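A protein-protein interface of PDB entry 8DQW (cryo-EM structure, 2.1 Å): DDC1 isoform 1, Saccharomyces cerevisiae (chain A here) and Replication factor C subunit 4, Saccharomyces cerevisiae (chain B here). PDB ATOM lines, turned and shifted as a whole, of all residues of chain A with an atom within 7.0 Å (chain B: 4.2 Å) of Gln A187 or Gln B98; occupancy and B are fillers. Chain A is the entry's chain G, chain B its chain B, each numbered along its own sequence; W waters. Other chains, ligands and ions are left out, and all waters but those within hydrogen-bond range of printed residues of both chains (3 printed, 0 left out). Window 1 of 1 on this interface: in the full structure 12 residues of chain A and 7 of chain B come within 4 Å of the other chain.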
ATOM      1  N   ASP A  62     -16.489  12.869  10.472  1.00  0.00           N
ATOM      2  CA  ASP A  62     -17.049  11.643   9.912  1.00  0.00           C
ATOM      3  C   ASP A  62     -18.557  11.758   9.721  1.00  0.00           C
ATOM      4  O   ASP A  62     -19.104  11.254   8.734  1.00  0.00           O
ATOM      5  CB  ASP A  62     -16.711  10.453  10.811  1.00  0.00           C
ATOM      6  CG  ASP A  62     -17.317  10.572  12.197  1.00  0.00           C
ATOM      7  OD1 ASP A  62     -17.886  11.637  12.517  1.00  0.00           O
ATOM      8  OD2 ASP A  62     -17.223   9.596  12.970  1.00  0.00           O
ATOM      9  N   ASP A  63     -19.242  12.416  10.651  1.00  0.00           N
ATOM     10  CA  ASP A  63     -20.691  12.560  10.619  1.00  0.00           C
ATOM     11  C   ASP A  63     -21.055  14.030  10.470  1.00  0.00           C
ATOM     12  O   ASP A  63     -20.508  14.883  11.177  1.00  0.00           O
ATOM     13  CB  ASP A  63     -21.321  11.983  11.889  1.00  0.00           C
ATOM     14  CG  ASP A  63     -21.791  10.552  11.708  1.00  0.00           C
ATOM     15  OD1 ASP A  63     -22.858  10.349  11.092  1.00  0.00           O
ATOM     16  OD2 ASP A  63     -21.094   9.630  12.180  1.00  0.00           O
ATOM     17  N   ASN A 110     -36.780  12.933  19.628  1.00  0.00           N
ATOM     18  CA  ASN A 110     -35.681  13.592  20.326  1.00  0.00           C
ATOM     19  C   ASN A 110     -35.019  14.667  19.472  1.00  0.00           C
ATOM     20  O   ASN A 110     -34.327  15.534  20.015  1.00  0.00           O
ATOM     21  CB  ASN A 110     -34.635  12.564  20.770  1.00  0.00           C
ATOM     22  CG  ASN A 110     -34.357  11.514  19.714  1.00  0.00           C
ATOM     23  OD1 ASN A 110     -35.251  11.116  18.967  1.00  0.00           O
ATOM     24  ND2 ASN A 110     -33.113  11.051  19.652  1.00  0.00           N
ATOM     25  N   GLY A 111     -35.213  14.631  18.153  1.00  0.00           N
ATOM     26  CA  GLY A 111     -34.669  15.659  17.286  1.00  0.00           C
ATOM     27  C   GLY A 111     -35.503  16.917  17.182  1.00  0.00           C
ATOM     28  O   GLY A 111     -35.025  17.916  16.638  1.00  0.00           O
ATOM     29  N   TYR A 126     -35.782  20.553  13.501  1.00  0.00           N
ATOM     30  CA  TYR A 126     -35.531  19.115  13.560  1.00  0.00           C
ATOM     31  C   TYR A 126     -34.093  18.841  13.149  1.00  0.00           C
ATOM     32  O   TYR A 126     -33.701  19.154  12.023  1.00  0.00           O
ATOM     33  CB  TYR A 126     -36.498  18.338  12.663  1.00  0.00           C
ATOM     34  CG  TYR A 126     -36.468  16.849  12.919  1.00  0.00           C
ATOM     35  CD1 TYR A 126     -36.958  16.323  14.107  1.00  0.00           C
ATOM     36  CD2 TYR A 126     -35.938  15.971  11.984  1.00  0.00           C
ATOM     37  CE1 TYR A 126     -36.929  14.966  14.354  1.00  0.00           C
ATOM     38  CE2 TYR A 126     -35.907  14.609  12.222  1.00  0.00           C
ATOM     39  CZ  TYR A 126     -36.404  14.113  13.409  1.00  0.00           C
ATOM     40  OH  TYR A 126     -36.377  12.760  13.657  1.00  0.00           O
ATOM     41  N   SER A 127     -33.319  18.235  14.044  1.00  0.00           N
ATOM     42  CA  SER A 127     -31.902  17.999  13.814  1.00  0.00           C
ATOM     43  C   SER A 127     -31.593  16.510  13.865  1.00  0.00           C
ATOM     44  O   SER A 127     -32.194  15.759  14.637  1.00  0.00           O
ATOM     45  CB  SER A 127     -31.048  18.740  14.848  1.00  0.00           C
ATOM     46  OG  SER A 127     -31.567  20.034  15.095  1.00  0.00           O
ATOM     47  N   PHE A 128     -30.647  16.090  13.028  1.00  0.00           N
ATOM     48  CA  PHE A 128     -30.199  14.705  13.019  1.00  0.00           C
ATOM     49  C   PHE A 128     -28.764  14.640  12.511  1.00  0.00           C
ATOM     50  O   PHE A 128     -28.217  15.614  11.989  1.00  0.00           O
ATOM     51  CB  PHE A 128     -31.121  13.813  12.178  1.00  0.00           C
ATOM     52  CG  PHE A 128     -31.276  14.258  10.752  1.00  0.00           C
ATOM     53  CD1 PHE A 128     -30.419  13.791   9.769  1.00  0.00           C
ATOM     54  CD2 PHE A 128     -32.289  15.129  10.390  1.00  0.00           C
ATOM     55  CE1 PHE A 128     -30.563  14.194   8.454  1.00  0.00           C
ATOM     56  CE2 PHE A 128     -32.439  15.535   9.077  1.00  0.00           C
ATOM     57  CZ  PHE A 128     -31.575  15.065   8.108  1.00  0.00           C
ATOM     58  N   ARG A 129     -28.153  13.474  12.701  1.00  0.00           N
ATOM     59  CA  ARG A 129     -26.780  13.205  12.306  1.00  0.00           C
ATOM     60  C   ARG A 129     -26.768  12.109  11.250  1.00  0.00           C
ATOM     61  O   ARG A 129     -27.531  11.143  11.342  1.00  0.00           O
ATOM     62  CB  ARG A 129     -25.940  12.785  13.520  1.00  0.00           C
ATOM     63  CG  ARG A 129     -24.576  12.229  13.179  1.00  0.00           C
ATOM     64  CD  ARG A 129     -23.703  12.100  14.418  1.00  0.00           C
ATOM     65  NE  ARG A 129     -24.316  11.257  15.438  1.00  0.00           N
ATOM     66  CZ  ARG A 129     -24.208   9.937  15.491  1.00  0.00           C
ATOM     67  NH1 ARG A 129     -23.522   9.259  14.584  1.00  0.00           N
ATOM     68  NH2 ARG A 129     -24.804   9.277  16.480  1.00  0.00           N
ATOM     69  N   VAL A 130     -25.906  12.258  10.245  1.00  0.00           N
ATOM     70  CA  VAL A 130     -25.842  11.315   9.133  1.00  0.00           C
ATOM     71  C   VAL A 130     -24.389  11.123   8.719  1.00  0.00           C
ATOM     72  O   VAL A 130     -23.595  12.069   8.735  1.00  0.00           O
ATOM     73  CB  VAL A 130     -26.694  11.795   7.937  1.00  0.00           C
ATOM     74  CG1 VAL A 130     -26.086  13.047   7.315  1.00  0.00           C
ATOM     75  CG2 VAL A 130     -26.834  10.686   6.905  1.00  0.00           C
ATOM     76  N   ASN A 131     -24.046   9.894   8.335  1.00  0.00           N
ATOM     77  CA  ASN A 131     -22.693   9.591   7.886  1.00  0.00           C
ATOM     78  C   ASN A 131     -22.318  10.479   6.704  1.00  0.00           C
ATOM     79  O   ASN A 131     -23.011  10.493   5.682  1.00  0.00           O
ATOM     80  CB  ASN A 131     -22.590   8.116   7.501  1.00  0.00           C
ATOM     81  CG  ASN A 131     -21.189   7.718   7.080  1.00  0.00           C
ATOM     82  OD1 ASN A 131     -20.704   8.127   6.026  1.00  0.00           O
ATOM     83  ND2 ASN A 131     -20.530   6.911   7.904  1.00  0.00           N
ATOM     84  N   ASN A 166     -36.369   6.719  10.988  1.00  0.00           N
ATOM     85  CA  ASN A 166     -35.017   7.247  11.172  1.00  0.00           C
ATOM     86  C   ASN A 166     -34.138   6.953   9.957  1.00  0.00           C
ATOM     87  O   ASN A 166     -33.008   6.478  10.077  1.00  0.00           O
ATOM     88  CB  ASN A 166     -34.384   6.694  12.451  1.00  0.00           C
ATOM     89  CG  ASN A 166     -35.151   7.086  13.695  1.00  0.00           C
ATOM     90  OD1 ASN A 166     -35.517   8.248  13.872  1.00  0.00           O
ATOM     91  ND2 ASN A 166     -35.412   6.114  14.558  1.00  0.00           N
ATOM     92  N   GLN A 185     -29.429   5.599   7.206  1.00  0.00           N
ATOM     93  CA  GLN A 185     -29.929   5.838   8.553  1.00  0.00           C
ATOM     94  C   GLN A 185     -29.444   7.185   9.083  1.00  0.00           C
ATOM     95  O   GLN A 185     -28.400   7.700   8.675  1.00  0.00           O
ATOM     96  CB  GLN A 185     -29.474   4.720   9.491  1.00  0.00           C
ATOM     97  CG  GLN A 185     -27.969   4.678   9.715  1.00  0.00           C
ATOM     98  CD  GLN A 185     -27.513   3.415  10.418  1.00  0.00           C
ATOM     99  OE1 GLN A 185     -28.132   2.359  10.287  1.00  0.00           O
ATOM    100  NE2 GLN A 185     -26.423   3.516  11.169  1.00  0.00           N
ATOM    101  N   PHE A 186     -30.221   7.759  10.001  1.00  0.00           N
ATOM    102  CA  PHE A 186     -29.814   8.961  10.715  1.00  0.00           C
ATOM    103  C   PHE A 186     -30.254   8.857  12.169  1.00  0.00           C
ATOM    104  O   PHE A 186     -31.187   8.124  12.507  1.00  0.00           O
ATOM    105  CB  PHE A 186     -30.381  10.238  10.069  1.00  0.00           C
ATOM    106  CG  PHE A 186     -31.873  10.401  10.217  1.00  0.00           C
ATOM    107  CD1 PHE A 186     -32.424  10.871  11.400  1.00  0.00           C
ATOM    108  CD2 PHE A 186     -32.721  10.112   9.162  1.00  0.00           C
ATOM    109  CE1 PHE A 186     -33.790  11.029  11.533  1.00  0.00           C
ATOM    110  CE2 PHE A 186     -34.088  10.271   9.289  1.00  0.00           C
ATOM    111  CZ  PHE A 186     -34.623  10.733  10.475  1.00  0.00           C
ATOM    112  N   GLN A 187     -29.567   9.608  13.027  1.00  0.00           N
ATOM    113  CA  GLN A 187     -29.842   9.630  14.460  1.00  0.00           C
ATOM    114  C   GLN A 187     -30.285  11.028  14.871  1.00  0.00           C
ATOM    115  O   GLN A 187     -29.521  11.991  14.677  1.00  0.00           O
ATOM    116  CB  GLN A 187     -28.603   9.209  15.255  1.00  0.00           C
ATOM    117  CG  GLN A 187     -28.180   7.770  15.022  1.00  0.00           C
ATOM    118  CD  GLN A 187     -27.261   7.620  13.824  1.00  0.00           C
ATOM    119  OE1 GLN A 187     -26.355   8.427  13.618  1.00  0.00           O
ATOM    120  NE2 GLN A 187     -27.491   6.581  13.029  1.00  0.00           N
ATOM    121  N   PRO A 188     -31.485  11.210  15.424  1.00  0.00           N
ATOM    122  CA  PRO A 188     -31.886  12.548  15.873  1.00  0.00           C
ATOM    123  C   PRO A 188     -30.977  13.062  16.980  1.00  0.00           C
ATOM    124  O   PRO A 188     -30.466  12.299  17.802  1.00  0.00           O
ATOM    125  CB  PRO A 188     -33.321  12.348  16.374  1.00  0.00           C
ATOM    126  CG  PRO A 188     -33.777  11.063  15.778  1.00  0.00           C
ATOM    127  CD  PRO A 188     -32.559  10.220  15.616  1.00  0.00           C
ATOM    128  N   ILE A 189     -30.774  14.378  16.989  1.00  0.00           N
ATOM    129  CA  ILE A 189     -29.917  15.022  17.979  1.00  0.00           C
ATOM    130  C   ILE A 189     -30.496  16.383  18.338  1.00  0.00           C
ATOM    131  O   ILE A 189     -31.495  16.819  17.756  1.00  0.00           O
ATOM    132  CB  ILE A 189     -28.474  15.168  17.463  1.00  0.00           C
ATOM    133  CG1 ILE A 189     -28.463  15.920  16.129  1.00  0.00           C
ATOM    134  CG2 ILE A 189     -27.818  13.801  17.320  1.00  0.00           C
ATOM    135  CD1 ILE A 189     -27.083  16.213  15.605  1.00  0.00           C
ATOM    136  N   LYS A 190     -29.869  17.060  19.292  1.00  0.00           N
ATOM    137  CA  LYS A 190     -30.237  18.417  19.659  1.00  0.00           C
ATOM    138  C   LYS A 190     -29.294  19.410  18.990  1.00  0.00           C
ATOM    139  O   LYS A 190     -28.133  19.099  18.713  1.00  0.00           O
ATOM    140  CB  LYS A 190     -30.202  18.604  21.178  1.00  0.00           C
ATOM    141  CG  LYS A 190     -31.218  17.757  21.927  1.00  0.00           C
ATOM    142  CD  LYS A 190     -32.642  18.108  21.526  1.00  0.00           C
ATOM    143  CE  LYS A 190     -33.619  17.854  22.660  1.00  0.00           C
ATOM    144  NZ  LYS A 190     -34.986  17.547  22.156  1.00  0.00           N
ATOM    145  N   LYS B  94     -19.739  -0.404  13.972  1.00  0.00           N
ATOM    146  CA  LYS B  94     -19.963   0.958  14.443  1.00  0.00           C
ATOM    147  C   LYS B  94     -21.301   1.498  13.953  1.00  0.00           C
ATOM    148  O   LYS B  94     -22.053   2.106  14.724  1.00  0.00           O
ATOM    149  CB  LYS B  94     -18.814   1.861  13.988  1.00  0.00           C
ATOM    150  CG  LYS B  94     -19.031   3.351  14.232  1.00  0.00           C
ATOM    151  CD  LYS B  94     -17.826   4.160  13.767  1.00  0.00           C
ATOM    152  CE  LYS B  94     -18.052   5.655  13.916  1.00  0.00           C
ATOM    153  NZ  LYS B  94     -18.285   6.057  15.328  1.00  0.00           N
ATOM    154  N   HIS B  95     -21.623   1.283  12.674  1.00  0.00           N
ATOM    155  CA  HIS B  95     -22.892   1.772  12.143  1.00  0.00           C
ATOM    156  C   HIS B  95     -24.071   1.042  12.773  1.00  0.00           C
ATOM    157  O   HIS B  95     -25.104   1.656  13.058  1.00  0.00           O
ATOM    158  CB  HIS B  95     -22.913   1.626  10.622  1.00  0.00           C
ATOM    159  CG  HIS B  95     -21.849   2.418   9.927  1.00  0.00           C
ATOM    160  ND1 HIS B  95     -21.253   2.000   8.757  1.00  0.00           N
ATOM    161  CD2 HIS B  95     -21.264   3.597  10.246  1.00  0.00           C
ATOM    162  CE1 HIS B  95     -20.353   2.890   8.381  1.00  0.00           C
ATOM    163  NE2 HIS B  95     -20.340   3.869   9.267  1.00  0.00           N
ATOM    164  N   PHE B  96     -23.939  -0.269  12.996  1.00  0.00           N
ATOM    165  CA  PHE B  96     -25.010  -1.003  13.663  1.00  0.00           C
ATOM    166  C   PHE B  96     -25.235  -0.480  15.076  1.00  0.00           C
ATOM    167  O   PHE B  96     -26.381  -0.301  15.504  1.00  0.00           O
ATOM    168  CB  PHE B  96     -24.687  -2.497  13.697  1.00  0.00           C
ATOM    169  CG  PHE B  96     -25.719  -3.319  14.418  1.00  0.00           C
ATOM    170  CD1 PHE B  96     -26.986  -3.490  13.886  1.00  0.00           C
ATOM    171  CD2 PHE B  96     -25.424  -3.911  15.636  1.00  0.00           C
ATOM    172  CE1 PHE B  96     -27.938  -4.243  14.550  1.00  0.00           C
ATOM    173  CE2 PHE B  96     -26.373  -4.665  16.305  1.00  0.00           C
ATOM    174  CZ  PHE B  96     -27.630  -4.831  15.761  1.00  0.00           C
ATOM    175  N   ALA B  97     -24.153  -0.222  15.812  1.00  0.00           N
ATOM    176  CA  ALA B  97     -24.288   0.269  17.178  1.00  0.00           C
ATOM    177  C   ALA B  97     -24.804   1.701  17.210  1.00  0.00           C
ATOM    178  O   ALA B  97     -25.423   2.111  18.199  1.00  0.00           O
ATOM    179  CB  ALA B  97     -22.946   0.172  17.905  1.00  0.00           C
ATOM    180  N   GLN B  98     -24.557   2.474  16.151  1.00  0.00           N
ATOM    181  CA  GLN B  98     -25.078   3.833  16.065  1.00  0.00           C
ATOM    182  C   GLN B  98     -26.551   3.877  15.683  1.00  0.00           C
ATOM    183  O   GLN B  98     -27.206   4.899  15.912  1.00  0.00           O
ATOM    184  CB  GLN B  98     -24.273   4.642  15.046  1.00  0.00           C
ATOM    185  CG  GLN B  98     -23.019   5.281  15.609  1.00  0.00           C
ATOM    186  CD  GLN B  98     -22.149   5.905  14.534  1.00  0.00           C
ATOM    187  OE1 GLN B  98     -22.182   5.491  13.375  1.00  0.00           O
ATOM    188  NE2 GLN B  98     -21.364   6.904  14.915  1.00  0.00           N
ATOM    189  N   LYS B  99     -27.081   2.801  15.107  1.00  0.00           N
ATOM    190  CA  LYS B  99     -28.465   2.794  14.657  1.00  0.00           C
ATOM    191  C   LYS B  99     -29.415   3.027  15.826  1.00  0.00           C
ATOM    192  O   LYS B  99     -29.258   2.442  16.901  1.00  0.00           O
ATOM    193  CB  LYS B  99     -28.788   1.462  13.982  1.00  0.00           C
ATOM    194  CG  LYS B  99     -29.991   1.504  13.056  1.00  0.00           C
ATOM    195  CD  LYS B  99     -30.723   0.173  13.030  1.00  0.00           C
ATOM    196  CE  LYS B  99     -29.974  -0.860  12.209  1.00  0.00           C
ATOM    197  NZ  LYS B  99     -30.347  -2.250  12.586  1.00  0.00           N
ATOM    198  N   LYS B 100     -30.407   3.887  15.610  1.00  0.00           N
ATOM    199  CA  LYS B 100     -31.444   4.150  16.600  1.00  0.00           C
ATOM    200  C   LYS B 100     -32.642   3.263  16.277  1.00  0.00           C
ATOM    201  O   LYS B 100     -33.351   3.498  15.294  1.00  0.00           O
ATOM    202  CB  LYS B 100     -31.842   5.623  16.614  1.00  0.00           C
ATOM    203  CG  LYS B 100     -32.691   5.994  17.820  1.00  0.00           C
ATOM    204  CD  LYS B 100     -33.776   6.988  17.468  1.00  0.00           C
ATOM    205  CE  LYS B 100     -34.725   7.193  18.634  1.00  0.00           C
ATOM    206  NZ  LYS B 100     -35.151   8.608  18.758  1.00  0.00           N
ATOM    207  N   TYR B 134     -21.295   2.829  22.937  1.00  0.00           N
ATOM    208  CA  TYR B 134     -22.634   2.406  22.536  1.00  0.00           C
ATOM    209  C   TYR B 134     -23.218   1.327  23.448  1.00  0.00           C
ATOM    210  O   TYR B 134     -24.077   0.552  23.021  1.00  0.00           O
ATOM    211  CB  TYR B 134     -22.614   1.920  21.088  1.00  0.00           C
ATOM    212  CG  TYR B 134     -21.975   2.906  20.138  1.00  0.00           C
ATOM    213  CD1 TYR B 134     -22.561   4.140  19.895  1.00  0.00           C
ATOM    214  CD2 TYR B 134     -20.779   2.612  19.497  1.00  0.00           C
ATOM    215  CE1 TYR B 134     -21.984   5.050  19.034  1.00  0.00           C
ATOM    216  CE2 TYR B 134     -20.192   3.519  18.632  1.00  0.00           C
ATOM    217  CZ  TYR B 134     -20.799   4.735  18.406  1.00  0.00           C
ATOM    218  OH  TYR B 134     -20.222   5.642  17.550  1.00  0.00           O
HETATM  219  O   HOH W   1     -26.388  -0.351  10.506  1.00  0.00           O
HETATM  220  O   HOH W   2     -30.588   5.063  12.870  1.00  0.00           O
HETATM  221  O   HOH W   3     -21.804   7.449  10.812  1.00  0.00           O
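Hydrophobic or aromatic side chains of chain A within 4 Å of the printed part of chain B: Pro A188. Hydrophobic or aromatic side chains of chain B within 4 Å of the printed part of chain A: His B95. Along chain B the printed residues that touch a printed residue of chain A span positions 95 to 100. Among the printed residues, 9 pairs touch across the chains.
Among the printed residues, merely in contact across the chains: Gln A185 with Lys B99 (3.4 Å), Asp A63 with Gln B98 (3.9 Å) and Pro A188 with Lys B100 (3.9 Å).
O of Asn A166 is in hydrogen-bond range of N of Phe A186 (3.1 Å). OH of Tyr B134 lies within hydrogen-bond range of NE2 of Gln B98 (3.1 Å). The backbone NH (N) of Arg A129 is in hydrogen-bond range of the backbone carbonyl oxygen (O) of Gln A187, at 2.8 Å. The side-chain amide nitrogen (NE2) of Gln B98 sits close to the side-chain amino group (NZ) of Lys B94 (3.2 Å). The backbone carbonyl oxygen (O) of Pro A188 sits at hydrogen-bond distance from the side-chain amide nitrogen (ND2) of Asn A110 (3.5 Å). OD1 of Asp A63 is in hydrogen-bond range of N of Asn A131.
Water W3 lies within hydrogen-bond range of the side-chain carboxylate (OD2) of Asp A63 (2.7 Å), the side-chain amide nitrogen (ND2) of Asn A131 (3.2 Å) and the side-chain amide oxygen (OE1) of Gln B98 (3.2 Å). Water W2 lies within hydrogen-bond range of the backbone NH of Lys B100 (3.0 Å), the backbone carbonyl oxygen of Phe A186 (3.1 Å) and the side-chain amide nitrogen of Gln A187 (3.5 Å). Water W1 lies within hydrogen-bond range of the side-chain amide oxygen (OE1) of Gln A185, the backbone carbonyl oxygen (O) of His B95 and the backbone NH (N) of Phe B96.
Of chain B, only Gln B98 (3.2 Å) comes within 4 Å of Gln A187. Gln B98 touches just these residues of chain A: Asp A63, Arg A129 and Gln A187. Printed residues of chain B within 4 Å of Asp A63: Gln B98 (3.9 Å). Of the printed residues of chain A, His B95 touches Asn A131 and Gln A185. Of the printed residues of chain A, Lys B100 touches Asn A110, Asn A166 and Pro A188. Tyr A126 touches none of the printed residues of chain B. The nearest printed residue of chain B that does not touch Asp A63 is Lys B94 (5.3 Å).
The backbone carbonyl oxygen (O) of His B95 is in hydrogen-bond range of the side-chain amide nitrogen (NE2) of Gln A185, 3.0 Å away. The backbone carbonyl oxygen (O) of Lys B100 sits at hydrogen-bond distance from the side-chain amide nitrogen (ND2) of Asn A166 (3.4 Å). NH1 of Arg A129 sits close to NE2 of Gln B98. OD1 of Asn A110 sits at hydrogen-bond distance from NZ of Lys B100. The side-chain amide nitrogen of Gln A187 sits close to the backbone carbonyl oxygen of Gln B98, 3.3 Å away. NE2 of His B95 sits at hydrogen-bond distance from ND2 of Asn A131 (3.3 Å).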
